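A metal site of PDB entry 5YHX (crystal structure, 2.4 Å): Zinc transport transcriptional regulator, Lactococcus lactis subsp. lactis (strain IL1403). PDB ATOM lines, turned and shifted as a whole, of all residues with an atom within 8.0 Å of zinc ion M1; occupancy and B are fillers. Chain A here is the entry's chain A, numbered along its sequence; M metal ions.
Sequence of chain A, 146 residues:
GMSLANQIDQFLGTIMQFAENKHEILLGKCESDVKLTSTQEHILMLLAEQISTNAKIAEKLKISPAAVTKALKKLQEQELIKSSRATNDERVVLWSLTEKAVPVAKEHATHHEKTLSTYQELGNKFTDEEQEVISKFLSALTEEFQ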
ATOM      1  N   HIS A  23      25.437  -2.553  34.160  1.00  0.00           N
ATOM      2  CA  HIS A  23      25.738  -3.440  33.060  1.00  0.00           C
ATOM      3  C   HIS A  23      26.899  -2.917  32.210  1.00  0.00           C
ATOM      4  O   HIS A  23      27.341  -3.601  31.296  1.00  0.00           O
ATOM      5  CB  HIS A  23      24.516  -3.594  32.164  1.00  0.00           C
ATOM      6  CG  HIS A  23      24.592  -2.825  30.884  1.00  0.00           C
ATOM      7  ND1 HIS A  23      24.008  -1.582  30.722  1.00  0.00           N
ATOM      8  CD2 HIS A  23      25.192  -3.110  29.707  1.00  0.00           C
ATOM      9  CE1 HIS A  23      24.233  -1.146  29.497  1.00  0.00           C
ATOM     10  NE2 HIS A  23      24.954  -2.053  28.854  1.00  0.00           N
ATOM     11  N   GLU A  24      27.351  -1.691  32.493  1.00  0.00           N
ATOM     12  CA  GLU A  24      28.470  -1.101  31.753  1.00  0.00           C
ATOM     13  C   GLU A  24      29.126   0.033  32.535  1.00  0.00           C
ATOM     14  O   GLU A  24      28.505   0.646  33.403  1.00  0.00           O
ATOM     15  CB  GLU A  24      28.014  -0.584  30.388  1.00  0.00           C
ATOM     16  CG  GLU A  24      27.202   0.705  30.404  1.00  0.00           C
ATOM     17  CD  GLU A  24      26.938   1.221  29.002  1.00  0.00           C
ATOM     18  OE1 GLU A  24      26.037   2.053  28.831  1.00  0.00           O
ATOM     19  OE2 GLU A  24      27.635   0.796  28.070  1.00  0.00           O
ATOM     20  N   ILE A  25      30.379   0.301  32.219  1.00  0.00           N
ATOM     21  CA  ILE A  25      31.156   1.326  32.907  1.00  0.00           C
ATOM     22  C   ILE A  25      31.004   2.690  32.244  1.00  0.00           C
ATOM     23  O   ILE A  25      31.456   2.893  31.122  1.00  0.00           O
ATOM     24  CB  ILE A  25      32.639   0.956  32.919  1.00  0.00           C
ATOM     25  CG1 ILE A  25      32.847  -0.435  33.506  1.00  0.00           C
ATOM     26  CG2 ILE A  25      33.431   1.941  33.757  1.00  0.00           C
ATOM     27  CD1 ILE A  25      32.562  -0.507  34.984  1.00  0.00           C
ATOM     28  N   LEU A  26      30.348   3.622  32.940  1.00  0.00           N
ATOM     29  CA  LEU A  26      30.292   5.018  32.519  1.00  0.00           C
ATOM     30  C   LEU A  26      30.792   5.876  33.671  1.00  0.00           C
ATOM     31  O   LEU A  26      30.466   5.599  34.822  1.00  0.00           O
ATOM     32  CB  LEU A  26      28.863   5.425  32.170  1.00  0.00           C
ATOM     33  CG  LEU A  26      28.193   4.729  30.972  1.00  0.00           C
ATOM     34  CD1 LEU A  26      26.681   5.049  30.967  1.00  0.00           C
ATOM     35  CD2 LEU A  26      28.867   5.163  29.681  1.00  0.00           C
ATOM     36  N   THR A  37      17.409   2.707  33.593  1.00  0.00           N
ATOM     37  CA  THR A  37      18.633   1.947  33.826  1.00  0.00           C
ATOM     38  C   THR A  37      19.644   2.203  32.701  1.00  0.00           C
ATOM     39  O   THR A  37      19.242   2.572  31.592  1.00  0.00           O
ATOM     40  CB  THR A  37      18.354   0.442  33.913  1.00  0.00           C
ATOM     41  OG1 THR A  37      18.086  -0.089  32.615  1.00  0.00           O
ATOM     42  CG2 THR A  37      17.154   0.194  34.823  1.00  0.00           C
ATOM     43  N   SER A  38      20.938   2.008  32.962  1.00  0.00           N
ATOM     44  CA  SER A  38      21.947   2.096  31.894  1.00  0.00           C
ATOM     45  C   SER A  38      21.511   1.307  30.660  1.00  0.00           C
ATOM     46  O   SER A  38      21.613   1.788  29.530  1.00  0.00           O
ATOM     47  CB  SER A  38      23.320   1.618  32.361  1.00  0.00           C
ATOM     48  OG  SER A  38      23.293   0.234  32.659  1.00  0.00           O
ATOM     49  N   THR A  39      20.991   0.094  30.864  1.00  0.00           N
ATOM     50  CA  THR A  39      20.614  -0.765  29.748  1.00  0.00           C
ATOM     51  C   THR A  39      19.495  -0.135  28.975  1.00  0.00           C
ATOM     52  O   THR A  39      19.545  -0.081  27.743  1.00  0.00           O
ATOM     53  CB  THR A  39      20.178  -2.198  30.186  1.00  0.00           C
ATOM     54  OG1 THR A  39      21.249  -2.837  30.881  1.00  0.00           O
ATOM     55  CG2 THR A  39      19.796  -3.059  28.980  1.00  0.00           C
ATOM     56  N   GLN A  40      18.473   0.347  29.679  1.00  0.00           N
ATOM     57  CA  GLN A  40      17.368   1.040  29.001  1.00  0.00           C
ATOM     58  C   GLN A  40      17.830   2.227  28.126  1.00  0.00           C
ATOM     59  O   GLN A  40      17.486   2.315  26.933  1.00  0.00           O
ATOM     60  CB  GLN A  40      16.330   1.509  30.013  1.00  0.00           C
ATOM     61  CG  GLN A  40      15.358   0.417  30.411  1.00  0.00           C
ATOM     62  CD  GLN A  40      14.840   0.565  31.833  1.00  0.00           C
ATOM     63  OE1 GLN A  40      14.966   1.617  32.460  1.00  0.00           O
ATOM     64  NE2 GLN A  40      14.265  -0.505  32.344  1.00  0.00           N
ATOM     65  N   GLU A  41      18.605   3.129  28.736  1.00  0.00           N
ATOM     66  CA  GLU A  41      19.084   4.316  28.048  1.00  0.00           C
ATOM     67  C   GLU A  41      19.952   3.908  26.876  1.00  0.00           C
ATOM     68  O   GLU A  41      19.836   4.457  25.783  1.00  0.00           O
ATOM     69  CB  GLU A  41      19.886   5.194  29.008  1.00  0.00           C
ATOM     70  CG  GLU A  41      19.025   6.041  29.913  1.00  0.00           C
ATOM     71  CD  GLU A  41      19.772   7.236  30.456  1.00  0.00           C
ATOM     72  OE1 GLU A  41      20.889   7.512  29.963  1.00  0.00           O
ATOM     73  OE2 GLU A  41      19.250   7.912  31.374  1.00  0.00           O
ATOM     74  N   HIS A  42      20.784   2.897  27.107  1.00  0.00           N
ATOM     75  CA  HIS A  42      21.609   2.369  26.030  1.00  0.00           C
ATOM     76  C   HIS A  42      20.787   1.893  24.830  1.00  0.00           C
ATOM     77  O   HIS A  42      21.179   2.132  23.697  1.00  0.00           O
ATOM     78  CB  HIS A  42      22.524   1.258  26.526  1.00  0.00           C
ATOM     79  CG  HIS A  42      23.652   0.972  25.589  1.00  0.00           C
ATOM     80  ND1 HIS A  42      24.942   1.389  25.842  1.00  0.00           N
ATOM     81  CD2 HIS A  42      23.677   0.374  24.375  1.00  0.00           C
ATOM     82  CE1 HIS A  42      25.725   1.023  24.848  1.00  0.00           C
ATOM     83  NE2 HIS A  42      24.974   0.408  23.937  1.00  0.00           N
ATOM     84  N   ILE A  43      19.656   1.245  25.067  1.00  0.00           N
ATOM     85  CA  ILE A  43      18.858   0.756  23.959  1.00  0.00           C
ATOM     86  C   ILE A  43      18.368   1.958  23.190  1.00  0.00           C
ATOM     87  O   ILE A  43      18.452   2.004  21.963  1.00  0.00           O
ATOM     88  CB  ILE A  43      17.670  -0.103  24.447  1.00  0.00           C
ATOM     89  CG1 ILE A  43      18.140  -1.503  24.855  1.00  0.00           C
ATOM     90  CG2 ILE A  43      16.616  -0.235  23.396  1.00  0.00           C
ATOM     91  CD1 ILE A  43      17.150  -2.252  25.684  1.00  0.00           C
ATOM     92  N   MET A  45      19.757   4.820  22.926  1.00  0.00           N
ATOM     93  CA  MET A  45      20.876   5.296  22.111  1.00  0.00           C
ATOM     94  C   MET A  45      21.127   4.458  20.856  1.00  0.00           C
ATOM     95  O   MET A  45      21.502   5.008  19.825  1.00  0.00           O
ATOM     96  CB  MET A  45      22.158   5.360  22.926  1.00  0.00           C
ATOM     97  CG  MET A  45      23.311   5.791  22.067  1.00  0.00           C
ATOM     98  SD  MET A  45      24.890   5.741  22.876  1.00  0.00           S
ATOM     99  CE  MET A  45      25.235   3.983  22.749  1.00  0.00           C
ATOM    100  N   LEU A  46      20.972   3.137  20.967  1.00  0.00           N
ATOM    101  CA  LEU A  46      21.135   2.263  19.804  1.00  0.00           C
ATOM    102  C   LEU A  46      20.052   2.565  18.775  1.00  0.00           C
ATOM    103  O   LEU A  46      20.345   2.646  17.590  1.00  0.00           O
ATOM    104  CB  LEU A  46      21.018   0.778  20.196  1.00  0.00           C
ATOM    105  CG  LEU A  46      22.140   0.226  21.054  1.00  0.00           C
ATOM    106  CD1 LEU A  46      21.880  -1.232  21.380  1.00  0.00           C
ATOM    107  CD2 LEU A  46      23.485   0.420  20.364  1.00  0.00           C
ATOM    108  N   LEU A  61      23.670  -5.718  22.621  1.00  0.00           N
ATOM    109  CA  LEU A  61      23.778  -5.697  24.064  1.00  0.00           C
ATOM    110  C   LEU A  61      24.360  -6.986  24.627  1.00  0.00           C
ATOM    111  O   LEU A  61      24.841  -7.007  25.768  1.00  0.00           O
ATOM    112  CB  LEU A  61      22.400  -5.480  24.658  1.00  0.00           C
ATOM    113  CG  LEU A  61      21.938  -4.035  24.563  1.00  0.00           C
ATOM    114  CD1 LEU A  61      20.434  -3.975  24.696  1.00  0.00           C
ATOM    115  CD2 LEU A  61      22.643  -3.216  25.630  1.00  0.00           C
ATOM    116  N   HIS A 108      22.725  10.040  26.831  1.00  0.00           N
ATOM    117  CA  HIS A 108      23.472   8.807  27.071  1.00  0.00           C
ATOM    118  C   HIS A 108      24.673   8.656  26.141  1.00  0.00           C
ATOM    119  O   HIS A 108      25.760   8.243  26.561  1.00  0.00           O
ATOM    120  CB  HIS A 108      22.556   7.601  26.911  1.00  0.00           C
ATOM    121  CG  HIS A 108      23.127   6.342  27.454  1.00  0.00           C
ATOM    122  ND1 HIS A 108      23.471   6.205  28.795  1.00  0.00           N
ATOM    123  CD2 HIS A 108      23.458   5.175  26.866  1.00  0.00           C
ATOM    124  CE1 HIS A 108      23.976   4.999  28.983  1.00  0.00           C
ATOM    125  NE2 HIS A 108      23.961   4.354  27.834  1.00  0.00           N
ATOM    126  N   ALA A 109      24.473   9.003  24.863  1.00  0.00           N
ATOM    127  CA  ALA A 109      25.591   9.070  23.900  1.00  0.00           C
ATOM    128  C   ALA A 109      26.675   9.999  24.424  1.00  0.00           C
ATOM    129  O   ALA A 109      27.877   9.691  24.365  1.00  0.00           O
ATOM    130  CB  ALA A 109      25.102   9.558  22.540  1.00  0.00           C
ATOM    131  N   HIS A 111      27.136  10.822  27.559  1.00  0.00           N
ATOM    132  CA  HIS A 111      27.750  10.189  28.708  1.00  0.00           C
ATOM    133  C   HIS A 111      28.866   9.254  28.199  1.00  0.00           C
ATOM    134  O   HIS A 111      29.977   9.227  28.730  1.00  0.00           O
ATOM    135  CB  HIS A 111      26.680   9.440  29.515  1.00  0.00           C
ATOM    136  CG  HIS A 111      27.066   9.184  30.936  1.00  0.00           C
ATOM    137  ND1 HIS A 111      26.164   8.773  31.892  1.00  0.00           N
ATOM    138  CD2 HIS A 111      28.274   9.247  31.564  1.00  0.00           C
ATOM    139  CE1 HIS A 111      26.788   8.604  33.051  1.00  0.00           C
ATOM    140  NE2 HIS A 111      28.065   8.887  32.874  1.00  0.00           N
ATOM    141  N   HIS A 112      28.582   8.510  27.136  1.00  0.00           N
ATOM    142  CA  HIS A 112      29.652   7.724  26.489  1.00  0.00           C
ATOM    143  C   HIS A 112      30.826   8.576  26.029  1.00  0.00           C
ATOM    144  O   HIS A 112      31.990   8.247  26.283  1.00  0.00           O
ATOM    145  CB  HIS A 112      29.106   6.846  25.359  1.00  0.00           C
ATOM    146  CG  HIS A 112      28.599   5.538  25.845  1.00  0.00           C
ATOM    147  ND1 HIS A 112      29.443   4.513  26.212  1.00  0.00           N
ATOM    148  CD2 HIS A 112      27.349   5.116  26.141  1.00  0.00           C
ATOM    149  CE1 HIS A 112      28.736   3.498  26.659  1.00  0.00           C
ATOM    150  NE2 HIS A 112      27.456   3.838  26.631  1.00  0.00           N
HETATM  151 ZN    ZN M   1      25.561   2.849  27.178  1.00  0.00          ZN
HETATM  152 ZN    ZN M   2      22.013   8.807  31.008  1.00  0.00          ZN
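ND1 of His 108 sits close to OE1 of Glu 41, at 3.1 Å.
Of the 18 residues printed, 4 come within 4 Å of zinc ion M1.
OE1 of Glu 24 binds zinc ion M1, 1.9 Å away.
ND1 of His 42 is bound to zinc ion M1.
Zinc ion M1 is bound by NE2 of His 112 (2.2 Å).
NE2 of His 108 is bound to zinc ion M1, at 2.3 Å.
Zinc ion M1 has four donor atoms within binding distance.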
